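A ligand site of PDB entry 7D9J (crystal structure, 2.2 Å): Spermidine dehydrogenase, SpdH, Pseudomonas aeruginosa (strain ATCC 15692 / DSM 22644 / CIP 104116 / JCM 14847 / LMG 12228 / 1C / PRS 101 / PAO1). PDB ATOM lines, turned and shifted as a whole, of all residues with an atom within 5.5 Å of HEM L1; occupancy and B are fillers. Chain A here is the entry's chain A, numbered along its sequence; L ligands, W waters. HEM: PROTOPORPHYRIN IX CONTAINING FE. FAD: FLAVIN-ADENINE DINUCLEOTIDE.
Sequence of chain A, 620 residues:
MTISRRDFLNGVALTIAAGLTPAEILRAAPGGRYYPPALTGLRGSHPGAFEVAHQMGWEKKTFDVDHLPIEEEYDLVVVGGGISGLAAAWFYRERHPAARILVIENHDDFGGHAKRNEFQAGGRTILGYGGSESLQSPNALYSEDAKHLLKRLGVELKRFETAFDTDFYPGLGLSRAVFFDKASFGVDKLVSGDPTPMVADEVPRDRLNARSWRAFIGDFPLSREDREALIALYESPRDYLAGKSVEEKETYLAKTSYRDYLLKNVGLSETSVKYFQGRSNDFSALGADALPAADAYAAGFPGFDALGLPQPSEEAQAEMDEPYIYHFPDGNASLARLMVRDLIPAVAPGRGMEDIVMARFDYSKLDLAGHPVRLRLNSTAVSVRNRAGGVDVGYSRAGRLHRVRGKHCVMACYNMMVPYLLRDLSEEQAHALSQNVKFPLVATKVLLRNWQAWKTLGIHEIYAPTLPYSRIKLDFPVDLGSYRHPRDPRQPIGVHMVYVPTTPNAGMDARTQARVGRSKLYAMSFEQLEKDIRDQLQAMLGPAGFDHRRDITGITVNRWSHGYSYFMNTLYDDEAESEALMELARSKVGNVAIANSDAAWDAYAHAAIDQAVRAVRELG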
ATOM      1  N   SER A  45      23.986  18.094  -4.845  1.00  0.00           N
ATOM      2  CA  SER A  45      24.515  19.024  -5.838  1.00  0.00           C
ATOM      3  C   SER A  45      23.692  20.309  -5.731  1.00  0.00           C
ATOM      4  O   SER A  45      22.715  20.510  -6.454  1.00  0.00           O
ATOM      5  CB  SER A  45      24.476  18.401  -7.229  1.00  0.00           C
ATOM      6  OG  SER A  45      25.547  17.465  -7.346  1.00  0.00           O
ATOM      7  N   HIS A  46      24.121  21.173  -4.812  1.00  0.00           N
ATOM      8  CA  HIS A  46      23.436  22.383  -4.359  1.00  0.00           C
ATOM      9  C   HIS A  46      23.595  23.528  -5.365  1.00  0.00           C
ATOM     10  O   HIS A  46      24.517  23.522  -6.180  1.00  0.00           O
ATOM     11  CB  HIS A  46      24.002  22.798  -3.004  1.00  0.00           C
ATOM     12  CG  HIS A  46      25.499  22.940  -3.017  1.00  0.00           C
ATOM     13  ND1 HIS A  46      26.135  24.044  -3.549  1.00  0.00           N
ATOM     14  CD2 HIS A  46      26.483  22.105  -2.600  1.00  0.00           C
ATOM     15  CE1 HIS A  46      27.446  23.895  -3.442  1.00  0.00           C
ATOM     16  NE2 HIS A  46      27.680  22.719  -2.876  1.00  0.00           N
ATOM     17  N   ALA A  49      27.025  24.691  -7.323  1.00  0.00           N
ATOM     18  CA  ALA A  49      27.963  23.621  -7.618  1.00  0.00           C
ATOM     19  C   ALA A  49      28.065  23.293  -9.093  1.00  0.00           C
ATOM     20  O   ALA A  49      29.106  22.771  -9.517  1.00  0.00           O
ATOM     21  CB  ALA A  49      27.588  22.336  -6.852  1.00  0.00           C
ATOM     22  N   PHE A  50      27.033  23.605  -9.890  1.00  0.00           N
ATOM     23  CA  PHE A  50      26.910  23.030 -11.221  1.00  0.00           C
ATOM     24  C   PHE A  50      26.832  24.042 -12.358  1.00  0.00           C
ATOM     25  O   PHE A  50      26.973  23.641 -13.524  1.00  0.00           O
ATOM     26  CB  PHE A  50      25.669  22.134 -11.302  1.00  0.00           C
ATOM     27  CG  PHE A  50      24.396  22.824 -10.878  1.00  0.00           C
ATOM     28  CD1 PHE A  50      23.668  23.587 -11.783  1.00  0.00           C
ATOM     29  CD2 PHE A  50      23.938  22.721  -9.572  1.00  0.00           C
ATOM     30  CE1 PHE A  50      22.495  24.234 -11.394  1.00  0.00           C
ATOM     31  CE2 PHE A  50      22.776  23.344  -9.168  1.00  0.00           C
ATOM     32  CZ  PHE A  50      22.049  24.113 -10.086  1.00  0.00           C
ATOM     33  N   ALA A  53      29.750  24.259 -14.776  1.00  0.00           N
ATOM     34  CA  ALA A  53      29.769  22.978 -15.469  1.00  0.00           C
ATOM     35  C   ALA A  53      28.699  22.895 -16.560  1.00  0.00           C
ATOM     36  O   ALA A  53      28.956  22.386 -17.664  1.00  0.00           O
ATOM     37  CB  ALA A  53      29.580  21.852 -14.451  1.00  0.00           C
ATOM     38  N   HIS A  54      27.484  23.412 -16.280  1.00  0.00           N
ATOM     39  CA  HIS A  54      26.446  23.434 -17.296  1.00  0.00           C
ATOM     40  C   HIS A  54      26.684  24.478 -18.376  1.00  0.00           C
ATOM     41  O   HIS A  54      26.249  24.284 -19.517  1.00  0.00           O
ATOM     42  CB  HIS A  54      25.088  23.673 -16.657  1.00  0.00           C
ATOM     43  CG  HIS A  54      24.554  22.460 -15.987  1.00  0.00           C
ATOM     44  ND1 HIS A  54      23.475  22.497 -15.131  1.00  0.00           N
ATOM     45  CD2 HIS A  54      24.945  21.178 -16.052  1.00  0.00           C
ATOM     46  CE1 HIS A  54      23.221  21.279 -14.690  1.00  0.00           C
ATOM     47  NE2 HIS A  54      24.106  20.457 -15.238  1.00  0.00           N
ATOM     48  N   GLY A  57      28.632  22.218 -20.511  1.00  0.00           N
ATOM     49  CA  GLY A  57      27.946  21.057 -21.070  1.00  0.00           C
ATOM     50  C   GLY A  57      26.708  21.392 -21.877  1.00  0.00           C
ATOM     51  O   GLY A  57      26.421  20.706 -22.867  1.00  0.00           O
ATOM     52  N   TRP A  58      25.963  22.419 -21.473  1.00  0.00           N
ATOM     53  CA  TRP A  58      24.725  22.785 -22.160  1.00  0.00           C
ATOM     54  C   TRP A  58      24.970  23.850 -23.231  1.00  0.00           C
ATOM     55  O   TRP A  58      24.597  23.665 -24.396  1.00  0.00           O
ATOM     56  CB  TRP A  58      23.690  23.279 -21.136  1.00  0.00           C
ATOM     57  CG  TRP A  58      23.196  22.249 -20.144  1.00  0.00           C
ATOM     58  CD1 TRP A  58      23.552  20.927 -20.081  1.00  0.00           C
ATOM     59  CD2 TRP A  58      22.242  22.454 -19.087  1.00  0.00           C
ATOM     60  NE1 TRP A  58      22.878  20.301 -19.042  1.00  0.00           N
ATOM     61  CE2 TRP A  58      22.074  21.212 -18.421  1.00  0.00           C
ATOM     62  CE3 TRP A  58      21.512  23.558 -18.635  1.00  0.00           C
ATOM     63  CZ2 TRP A  58      21.203  21.053 -17.340  1.00  0.00           C
ATOM     64  CZ3 TRP A  58      20.661  23.407 -17.557  1.00  0.00           C
ATOM     65  CH2 TRP A  58      20.517  22.153 -16.925  1.00  0.00           C
ATOM     66  N   ASN A 106      34.135  21.284  -6.963  1.00  0.00           N
ATOM     67  CA  ASN A 106      33.138  22.297  -7.300  1.00  0.00           C
ATOM     68  C   ASN A 106      32.030  22.457  -6.264  1.00  0.00           C
ATOM     69  O   ASN A 106      31.413  23.522  -6.219  1.00  0.00           O
ATOM     70  CB  ASN A 106      32.512  22.003  -8.671  1.00  0.00           C
ATOM     71  CG  ASN A 106      31.800  20.671  -8.697  1.00  0.00           C
ATOM     72  OD1 ASN A 106      32.402  19.637  -8.455  1.00  0.00           O
ATOM     73  ND2 ASN A 106      30.489  20.691  -8.934  1.00  0.00           N
ATOM     74  N   HIS A 107      31.736  21.444  -5.458  1.00  0.00           N
ATOM     75  CA  HIS A 107      30.754  21.614  -4.395  1.00  0.00           C
ATOM     76  C   HIS A 107      31.340  22.453  -3.270  1.00  0.00           C
ATOM     77  O   HIS A 107      32.548  22.748  -3.239  1.00  0.00           O
ATOM     78  CB  HIS A 107      30.302  20.263  -3.846  1.00  0.00           C
ATOM     79  CG  HIS A 107      29.419  19.482  -4.775  1.00  0.00           C
ATOM     80  ND1 HIS A 107      29.920  18.663  -5.760  1.00  0.00           N
ATOM     81  CD2 HIS A 107      28.074  19.379  -4.842  1.00  0.00           C
ATOM     82  CE1 HIS A 107      28.918  18.106  -6.413  1.00  0.00           C
ATOM     83  NE2 HIS A 107      27.791  18.522  -5.879  1.00  0.00           N
ATOM     84  N   TYR A 414      33.329  13.458 -12.564  1.00  0.00           N
ATOM     85  CA  TYR A 414      32.401  12.726 -13.399  1.00  0.00           C
ATOM     86  C   TYR A 414      33.029  12.536 -14.785  1.00  0.00           C
ATOM     87  O   TYR A 414      33.548  13.483 -15.365  1.00  0.00           O
ATOM     88  CB  TYR A 414      31.070  13.481 -13.542  1.00  0.00           C
ATOM     89  CG  TYR A 414      30.347  13.916 -12.262  1.00  0.00           C
ATOM     90  CD1 TYR A 414      30.447  13.196 -11.073  1.00  0.00           C
ATOM     91  CD2 TYR A 414      29.532  15.039 -12.282  1.00  0.00           C
ATOM     92  CE1 TYR A 414      29.753  13.612  -9.921  1.00  0.00           C
ATOM     93  CE2 TYR A 414      28.838  15.455 -11.129  1.00  0.00           C
ATOM     94  CZ  TYR A 414      28.956  14.741  -9.968  1.00  0.00           C
ATOM     95  OH  TYR A 414      28.251  15.175  -8.870  1.00  0.00           O
ATOM     96  N   MET A 416      31.761  11.981 -17.744  1.00  0.00           N
ATOM     97  CA  MET A 416      31.176  12.756 -18.841  1.00  0.00           C
ATOM     98  C   MET A 416      31.546  14.225 -18.781  1.00  0.00           C
ATOM     99  O   MET A 416      31.356  14.926 -19.769  1.00  0.00           O
ATOM    100  CB  MET A 416      29.639  12.663 -18.933  1.00  0.00           C
ATOM    101  CG  MET A 416      28.847  12.355 -17.686  1.00  0.00           C
ATOM    102  SD  MET A 416      28.875  13.331 -16.196  1.00  0.00           S
ATOM    103  CE  MET A 416      28.816  15.032 -16.680  1.00  0.00           C
ATOM    104  N   MET A 417      32.054  14.694 -17.644  1.00  0.00           N
ATOM    105  CA  MET A 417      32.595  16.052 -17.580  1.00  0.00           C
ATOM    106  C   MET A 417      33.942  16.165 -18.289  1.00  0.00           C
ATOM    107  O   MET A 417      34.288  17.260 -18.767  1.00  0.00           O
ATOM    108  CB  MET A 417      32.750  16.487 -16.121  1.00  0.00           C
ATOM    109  CG  MET A 417      33.240  17.929 -15.941  1.00  0.00           C
ATOM    110  SD  MET A 417      31.954  19.189 -15.835  1.00  0.00           S
ATOM    111  CE  MET A 417      31.990  19.948 -17.467  1.00  0.00           C
ATOM    112  N   TYR A 420      34.809  18.129 -21.700  1.00  0.00           N
ATOM    113  CA  TYR A 420      34.717  19.573 -21.641  1.00  0.00           C
ATOM    114  C   TYR A 420      35.966  20.218 -21.051  1.00  0.00           C
ATOM    115  O   TYR A 420      36.155  21.431 -21.245  1.00  0.00           O
ATOM    116  CB  TYR A 420      33.463  19.959 -20.851  1.00  0.00           C
ATOM    117  CG  TYR A 420      32.226  19.457 -21.566  1.00  0.00           C
ATOM    118  CD1 TYR A 420      31.732  20.104 -22.688  1.00  0.00           C
ATOM    119  CD2 TYR A 420      31.602  18.285 -21.169  1.00  0.00           C
ATOM    120  CE1 TYR A 420      30.619  19.626 -23.384  1.00  0.00           C
ATOM    121  CE2 TYR A 420      30.492  17.810 -21.841  1.00  0.00           C
ATOM    122  CZ  TYR A 420      30.008  18.470 -22.957  1.00  0.00           C
ATOM    123  OH  TYR A 420      28.900  17.981 -23.619  1.00  0.00           O
ATOM    124  N   SER A 434      31.751  10.272 -22.819  1.00  0.00           N
ATOM    125  CA  SER A 434      30.422  10.862 -22.800  1.00  0.00           C
ATOM    126  C   SER A 434      29.329   9.807 -22.630  1.00  0.00           C
ATOM    127  O   SER A 434      28.192  10.169 -22.286  1.00  0.00           O
ATOM    128  CB  SER A 434      30.169  11.636 -24.091  1.00  0.00           C
ATOM    129  OG  SER A 434      29.871  10.736 -25.146  1.00  0.00           O
ATOM    130  N   VAL A 437      26.725   7.711 -18.750  1.00  0.00           N
ATOM    131  CA  VAL A 437      25.574   8.517 -18.401  1.00  0.00           C
ATOM    132  C   VAL A 437      25.167   8.108 -16.987  1.00  0.00           C
ATOM    133  O   VAL A 437      24.616   7.019 -16.796  1.00  0.00           O
ATOM    134  CB  VAL A 437      24.424   8.314 -19.401  1.00  0.00           C
ATOM    135  CG1 VAL A 437      23.189   9.110 -18.985  1.00  0.00           C
ATOM    136  CG2 VAL A 437      24.875   8.666 -20.805  1.00  0.00           C
ATOM    137  N   ARG A 515      18.862  10.434 -18.168  1.00  0.00           N
ATOM    138  CA  ARG A 515      18.827  11.807 -18.656  1.00  0.00           C
ATOM    139  C   ARG A 515      17.467  12.446 -18.412  1.00  0.00           C
ATOM    140  O   ARG A 515      17.390  13.595 -17.984  1.00  0.00           O
ATOM    141  CB  ARG A 515      19.171  11.852 -20.147  1.00  0.00           C
ATOM    142  CG  ARG A 515      20.605  11.434 -20.517  1.00  0.00           C
ATOM    143  CD  ARG A 515      20.828  11.601 -22.027  1.00  0.00           C
ATOM    144  NE  ARG A 515      22.114  11.105 -22.531  1.00  0.00           N
ATOM    145  CZ  ARG A 515      22.241   9.983 -23.244  1.00  0.00           C
ATOM    146  NH1 ARG A 515      21.172   9.231 -23.514  1.00  0.00           N
ATOM    147  NH2 ARG A 515      23.435   9.606 -23.674  1.00  0.00           N
ATOM    148  N   ARG A 518      17.047  13.359 -14.779  1.00  0.00           N
ATOM    149  CA  ARG A 518      17.708  14.630 -14.498  1.00  0.00           C
ATOM    150  C   ARG A 518      16.894  15.813 -14.991  1.00  0.00           C
ATOM    151  O   ARG A 518      16.880  16.863 -14.339  1.00  0.00           O
ATOM    152  CB  ARG A 518      19.101  14.658 -15.124  1.00  0.00           C
ATOM    153  CG  ARG A 518      20.196  14.376 -14.143  1.00  0.00           C
ATOM    154  CD  ARG A 518      21.545  14.584 -14.806  1.00  0.00           C
ATOM    155  NE  ARG A 518      21.816  13.628 -15.878  1.00  0.00           N
ATOM    156  CZ  ARG A 518      22.182  12.369 -15.674  1.00  0.00           C
ATOM    157  NH1 ARG A 518      22.264  11.892 -14.433  1.00  0.00           N
ATOM    158  NH2 ARG A 518      22.442  11.564 -16.708  1.00  0.00           N
ATOM    159  N   SER A 519      16.212  15.685 -16.144  1.00  0.00           N
ATOM    160  CA  SER A 519      15.319  16.759 -16.573  1.00  0.00           C
ATOM    161  C   SER A 519      14.229  17.000 -15.556  1.00  0.00           C
ATOM    162  O   SER A 519      13.911  18.154 -15.240  1.00  0.00           O
ATOM    163  CB  SER A 519      14.692  16.442 -17.945  1.00  0.00           C
ATOM    164  OG  SER A 519      15.681  16.381 -18.964  1.00  0.00           O
ATOM    165  N   LEU A 521      14.328  16.330 -12.318  1.00  0.00           N
ATOM    166  CA  LEU A 521      14.922  16.949 -11.145  1.00  0.00           C
ATOM    167  C   LEU A 521      15.205  18.417 -11.389  1.00  0.00           C
ATOM    168  O   LEU A 521      15.059  19.244 -10.484  1.00  0.00           O
ATOM    169  CB  LEU A 521      16.212  16.222 -10.732  1.00  0.00           C
ATOM    170  CG  LEU A 521      16.036  14.898  -9.977  1.00  0.00           C
ATOM    171  CD1 LEU A 521      17.380  14.259  -9.625  1.00  0.00           C
ATOM    172  CD2 LEU A 521      15.165  15.114  -8.728  1.00  0.00           C
ATOM    173  N   TYR A 522      15.598  18.776 -12.602  1.00  0.00           N
ATOM    174  CA  TYR A 522      15.912  20.160 -12.894  1.00  0.00           C
ATOM    175  C   TYR A 522      14.670  21.047 -12.863  1.00  0.00           C
ATOM    176  O   TYR A 522      14.770  22.248 -12.585  1.00  0.00           O
ATOM    177  CB  TYR A 522      16.625  20.232 -14.243  1.00  0.00           C
ATOM    178  CG  TYR A 522      17.120  21.610 -14.617  1.00  0.00           C
ATOM    179  CD1 TYR A 522      18.250  22.143 -14.019  1.00  0.00           C
ATOM    180  CD2 TYR A 522      16.453  22.365 -15.560  1.00  0.00           C
ATOM    181  CE1 TYR A 522      18.705  23.404 -14.361  1.00  0.00           C
ATOM    182  CE2 TYR A 522      16.905  23.617 -15.913  1.00  0.00           C
ATOM    183  CZ  TYR A 522      18.025  24.137 -15.321  1.00  0.00           C
ATOM    184  OH  TYR A 522      18.466  25.394 -15.665  1.00  0.00           O
ATOM    185  N   ARG A 559      20.544  16.079  -3.405  1.00  0.00           N
ATOM    186  CA  ARG A 559      20.106  15.889  -4.790  1.00  0.00           C
ATOM    187  C   ARG A 559      21.324  15.473  -5.618  1.00  0.00           C
ATOM    188  O   ARG A 559      22.182  16.293  -5.946  1.00  0.00           O
ATOM    189  CB  ARG A 559      19.468  17.173  -5.300  1.00  0.00           C
ATOM    190  CG  ARG A 559      19.196  17.187  -6.797  1.00  0.00           C
ATOM    191  CD  ARG A 559      18.592  18.508  -7.228  1.00  0.00           C
ATOM    192  NE  ARG A 559      19.472  19.639  -6.998  1.00  0.00           N
ATOM    193  CZ  ARG A 559      19.086  20.916  -7.118  1.00  0.00           C
ATOM    194  NH1 ARG A 559      17.832  21.195  -7.452  1.00  0.00           N
ATOM    195  NH2 ARG A 559      19.957  21.882  -6.910  1.00  0.00           N
ATOM    196  N   SER A 561      21.934  14.604  -8.846  1.00  0.00           N
ATOM    197  CA  SER A 561      21.498  14.576 -10.240  1.00  0.00           C
ATOM    198  C   SER A 561      22.427  13.702 -11.076  1.00  0.00           C
ATOM    199  O   SER A 561      21.994  13.023 -12.010  1.00  0.00           O
ATOM    200  CB  SER A 561      21.442  15.991 -10.796  1.00  0.00           C
ATOM    201  OG  SER A 561      20.578  16.789  -9.996  1.00  0.00           O
ATOM    202  N   HIS A 562      23.712  13.712 -10.736  1.00  0.00           N
ATOM    203  CA  HIS A 562      24.688  12.804 -11.329  1.00  0.00           C
ATOM    204  C   HIS A 562      25.156  11.898 -10.201  1.00  0.00           C
ATOM    205  O   HIS A 562      26.127  12.188  -9.499  1.00  0.00           O
ATOM    206  CB  HIS A 562      25.810  13.599 -11.964  1.00  0.00           C
ATOM    207  CG  HIS A 562      25.356  14.422 -13.126  1.00  0.00           C
ATOM    208  ND1 HIS A 562      25.236  13.906 -14.402  1.00  0.00           N
ATOM    209  CD2 HIS A 562      24.952  15.711 -13.205  1.00  0.00           C
ATOM    210  CE1 HIS A 562      24.786  14.844 -15.218  1.00  0.00           C
ATOM    211  NE2 HIS A 562      24.622  15.952 -14.528  1.00  0.00           N
HETATM  212  CHA HEM L   1      24.027  17.167 -18.134  1.00  0.00           C
HETATM  213  CHB HEM L   1      20.819  18.298 -14.652  1.00  0.00           C
HETATM  214  CHC HEM L   1      24.496  18.994 -11.556  1.00  0.00           C
HETATM  215  CHD HEM L   1      27.627  18.417 -15.137  1.00  0.00           C
HETATM  216  C1A HEM L   1      22.864  17.394 -17.434  1.00  0.00           C
HETATM  217  C2A HEM L   1      21.528  17.285 -18.001  1.00  0.00           C
HETATM  218  C3A HEM L   1      20.651  17.602 -17.047  1.00  0.00           C
HETATM  219  C4A HEM L   1      21.391  17.926 -15.855  1.00  0.00           C
HETATM  220  CMA HEM L   1      19.101  17.639 -17.139  1.00  0.00           C
HETATM  221  CAA HEM L   1      21.260  16.855 -19.459  1.00  0.00           C
HETATM  222  CBA HEM L   1      21.092  15.332 -19.521  1.00  0.00           C
HETATM  223  CGA HEM L   1      22.431  14.631 -19.508  1.00  0.00           C
HETATM  224  O1A HEM L   1      23.224  14.861 -20.465  1.00  0.00           O
HETATM  225  O2A HEM L   1      22.719  13.827 -18.571  1.00  0.00           O
HETATM  226  C1B HEM L   1      21.539  18.591 -13.513  1.00  0.00           C
HETATM  227  C2B HEM L   1      20.989  18.996 -12.233  1.00  0.00           C
HETATM  228  C3B HEM L   1      22.048  19.157 -11.409  1.00  0.00           C
HETATM  229  C4B HEM L   1      23.262  18.904 -12.140  1.00  0.00           C
HETATM  230  CMB HEM L   1      19.481  19.158 -11.881  1.00  0.00           C
HETATM  231  CAB HEM L   1      22.137  19.612  -9.946  1.00  0.00           C
HETATM  232  CBB HEM L   1      21.257  20.452  -9.412  1.00  0.00           C
HETATM  233  C1C HEM L   1      25.682  18.872 -12.212  1.00  0.00           C
HETATM  234  C2C HEM L   1      27.026  18.949 -11.642  1.00  0.00           C
HETATM  235  C3C HEM L   1      27.873  18.764 -12.674  1.00  0.00           C
HETATM  236  C4C HEM L   1      27.106  18.609 -13.890  1.00  0.00           C
HETATM  237  CMC HEM L   1      27.365  19.147 -10.137  1.00  0.00           C
HETATM  238  CAC HEM L   1      29.418  18.759 -12.729  1.00  0.00           C
HETATM  239  CBC HEM L   1      30.199  19.330 -11.817  1.00  0.00           C
HETATM  240  C1D HEM L   1      26.927  18.110 -16.281  1.00  0.00           C
HETATM  241  C2D HEM L   1      27.457  18.023 -17.615  1.00  0.00           C
HETATM  242  C3D HEM L   1      26.474  17.680 -18.454  1.00  0.00           C
HETATM  243  C4D HEM L   1      25.273  17.534 -17.673  1.00  0.00           C
HETATM  244  CMD HEM L   1      28.940  18.290 -17.991  1.00  0.00           C
HETATM  245  CAD HEM L   1      26.579  17.450 -19.974  1.00  0.00           C
HETATM  246  CBD HEM L   1      26.604  15.932 -20.167  1.00  0.00           C
HETATM  247  CGD HEM L   1      27.192  15.566 -21.513  1.00  0.00           C
HETATM  248  O1D HEM L   1      27.177  16.425 -22.432  1.00  0.00           O
HETATM  249  O2D HEM L   1      27.683  14.411 -21.672  1.00  0.00           O
HETATM  250  NA  HEM L   1      22.746  17.800 -16.118  1.00  0.00           N
HETATM  251  NB  HEM L   1      22.923  18.543 -13.428  1.00  0.00           N
HETATM  252  NC  HEM L   1      25.767  18.662 -13.571  1.00  0.00           N
HETATM  253  ND  HEM L   1      25.580  17.806 -16.355  1.00  0.00           N
HETATM  254 FE   HEM L   1      24.347  18.270 -14.850  1.00  0.00          FE
HETATM  255  PA  FAD L   2      32.077  11.543  -6.662  1.00  0.00           P
HETATM  256  O1A FAD L   2      31.864  11.303  -5.219  1.00  0.00           O
HETATM  257  O2A FAD L   2      30.831  11.887  -7.474  1.00  0.00           O
HETATM  258  O5B FAD L   2      33.215  12.661  -6.810  1.00  0.00           O
HETATM  259  C5B FAD L   2      33.460  13.335  -8.065  1.00  0.00           C
HETATM  260  C4B FAD L   2      33.431  14.821  -7.794  1.00  0.00           C
HETATM  261  O4B FAD L   2      33.967  15.550  -8.930  1.00  0.00           O
HETATM  262  C3B FAD L   2      32.042  15.400  -7.508  1.00  0.00           C
HETATM  263  O3B FAD L   2      31.982  16.106  -6.272  1.00  0.00           O
HETATM  264  C2B FAD L   2      31.802  16.350  -8.687  1.00  0.00           C
HETATM  265  O2B FAD L   2      30.967  17.453  -8.357  1.00  0.00           O
HETATM  266  C1B FAD L   2      33.238  16.761  -8.985  1.00  0.00           C
HETATM  267  N9A FAD L   2      33.425  17.448 -10.268  1.00  0.00           N
HETATM  268  C8A FAD L   2      32.711  17.278 -11.426  1.00  0.00           C
HETATM  269  N7A FAD L   2      33.070  18.084 -12.396  1.00  0.00           N
HETATM  270  C5A FAD L   2      34.059  18.871 -11.825  1.00  0.00           C
HETATM  271  C6A FAD L   2      34.849  19.935 -12.318  1.00  0.00           C
HETATM  272  N6A FAD L   2      34.761  20.412 -13.567  1.00  0.00           N
HETATM  273  N1A FAD L   2      35.749  20.497 -11.478  1.00  0.00           N
HETATM  274  C2A FAD L   2      35.844  20.024 -10.233  1.00  0.00           C
HETATM  275  N3A FAD L   2      35.168  19.035  -9.657  1.00  0.00           N
HETATM  276  C4A FAD L   2      34.289  18.487 -10.513  1.00  0.00           C
HETATM  277  N1  FAD L   2      28.910   3.317  -3.008  1.00  0.00           N
HETATM  278  C2  FAD L   2      29.191   2.339  -2.097  1.00  0.00           C
HETATM  279  O2  FAD L   2      30.221   1.653  -2.167  1.00  0.00           O
HETATM  280  N3  FAD L   2      28.297   2.082  -1.073  1.00  0.00           N
HETATM  281  C4  FAD L   2      27.098   2.737  -0.843  1.00  0.00           C
HETATM  282  O4  FAD L   2      26.393   2.419   0.099  1.00  0.00           O
HETATM  283  C4X FAD L   2      26.820   3.795  -1.812  1.00  0.00           C
HETATM  284  N5  FAD L   2      25.720   4.475  -1.673  1.00  0.00           N
HETATM  285  C5X FAD L   2      25.452   5.493  -2.589  1.00  0.00           C
HETATM  286  C6  FAD L   2      24.271   6.248  -2.455  1.00  0.00           C
HETATM  287  C7  FAD L   2      23.965   7.257  -3.354  1.00  0.00           C
HETATM  288  C7M FAD L   2      22.685   8.055  -3.186  1.00  0.00           C
HETATM  289  C8  FAD L   2      24.858   7.556  -4.399  1.00  0.00           C
HETATM  290  C8M FAD L   2      24.559   8.648  -5.387  1.00  0.00           C
HETATM  291  C9  FAD L   2      26.026   6.820  -4.534  1.00  0.00           C
HETATM  292  C9A FAD L   2      26.331   5.788  -3.637  1.00  0.00           C
HETATM  293  N10 FAD L   2      27.520   5.034  -3.739  1.00  0.00           N
HETATM  294  C10 FAD L   2      27.786   4.014  -2.847  1.00  0.00           C
HETATM  295  C1' FAD L   2      28.456   5.234  -4.868  1.00  0.00           C
HETATM  296  C2' FAD L   2      29.310   6.482  -4.760  1.00  0.00           C
HETATM  297  O2' FAD L   2      29.356   7.068  -6.056  1.00  0.00           O
HETATM  298  C3' FAD L   2      30.718   6.072  -4.332  1.00  0.00           C
HETATM  299  O3' FAD L   2      30.611   5.415  -3.085  1.00  0.00           O
HETATM  300  C4' FAD L   2      31.736   7.219  -4.225  1.00  0.00           C
HETATM  301  O4' FAD L   2      31.184   8.209  -3.348  1.00  0.00           O
HETATM  302  C5' FAD L   2      32.055   7.803  -5.588  1.00  0.00           C
HETATM  303  O5' FAD L   2      33.238   8.623  -5.481  1.00  0.00           O
HETATM  304  P   FAD L   2      33.859   9.306  -6.769  1.00  0.00           P
HETATM  305  O1P FAD L   2      34.060   8.217  -7.823  1.00  0.00           O
HETATM  306  O2P FAD L   2      35.042  10.115  -6.314  1.00  0.00           O
HETATM  307  O3P FAD L   2      32.720  10.261  -7.346  1.00  0.00           O
HETATM  308  O   HOH W   1      30.285  14.085 -22.220  1.00  0.00           O
HETATM  309  O   HOH W   2      24.255  12.726 -21.827  1.00  0.00           O
HETATM  310  O   HOH W   3      24.946  12.565 -18.525  1.00  0.00           O
HETATM  311  O   HOH W   4      26.663  12.041 -20.896  1.00  0.00           O
HETATM  312  O   HOH W   5      25.295  18.158 -23.266  1.00  0.00           O
HETATM  313  O   HOH W   6      22.875  16.185 -22.616  1.00  0.00           O
HETATM  314  O   HOH W   7      26.888  13.845 -24.383  1.00  0.00           O
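An iron atom (FE) of HEM L1 is bound by a ring nitrogen (NE2) of His 54 (2.2 Å).
FE of HEM L1 is bound by NE2 of His 562 (2.4 Å).
The side-chain hydroxyl of Tyr 420 lies within hydrogen-bond range of an oxygen (O1D) of HEM L1 (2.6 Å).
O2A of HEM L1 lies within salt-bridge range of NE of Arg 518 (2.8 Å).
An oxygen (O2B) of FAD L2 lies within hydrogen-bond range of the side-chain amide oxygen of Asn 106 (2.6 Å).
A ring nitrogen (ND1) of His 107 sits close to an oxygen (O2B) of FAD L2 (3.1 Å).
The guanidinium group (NH1) of Arg 518 lies within hydrogen-bond range of the backbone carbonyl oxygen (O) of Ser 561 (2.7 Å).
The backbone NH (N) of Ser 45 lies within hydrogen-bond range of the backbone carbonyl oxygen (O) of Arg 559.
ND2 of Asn 106 lies within hydrogen-bond range of O of Ala 49 (2.6 Å).
OG of Ser 45 sits at hydrogen-bond distance from NE2 of His 107.
The backbone carbonyl oxygen (O) of Arg 515 is in hydrogen-bond range of the side-chain hydroxyl (OG) of Ser 519.
Water W3 lies within hydrogen-bond range of an oxygen (O2A) of HEM L1 (2.6 Å) and the guanidinium group (NH2) of Arg 518 (3.3 Å).
Water W1 lies within hydrogen-bond range of O2D of HEM L1 and O of Met 416.
Water W5 lies within hydrogen-bond range of O1D of HEM L1 (2.7 Å) and O of Gly 57 (2.8 Å).
Water W4 lies within hydrogen-bond range of an oxygen (O2D) of HEM L1 (2.7 Å) and the backbone carbonyl oxygen (O) of Ser 434 (2.8 Å).
Water W2 lies within hydrogen-bond range of O1A of HEM L1 (2.7 Å) and NE of Arg 515 (2.8 Å).
Ser 45 touches HEM L1.
CE2 of Phe 50 touches CBB of HEM L1 (3.3 Å).
CB of Ala 53 touches CAC of HEM L1 (3.5 Å).
NE1 of Trp 58 touches C1A of HEM L1, 3.3 Å away.
ND2 of Asn 106 touches CBC of HEM L1, 3.2 Å away.
CE2 of Tyr 414 touches CAC of HEM L1, 3.7 Å away.
CE of Met 416 touches C2D of HEM L1, 3.4 Å away.
CE of Met 417 touches CMD of HEM L1, at 3.5 Å.
Arg 515 touches HEM L1.
Ser 519 touches HEM L1 (N to CMA, 3.6 Å).
Tyr 522 touches HEM L1.
Arg 559 touches HEM L1.
OG of Ser 561 touches C3B of HEM L1 (3.1 Å).
Hydrophobic or aromatic side chains within 4 Å of HEM L1: Phe 50, Ala 53, His 54, Trp 58, Tyr 414, Met 416, Met 417, Tyr 420, Tyr 522 and His 562.
Of the 24 residues printed, 17 come within 4 Å of HEM L1.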
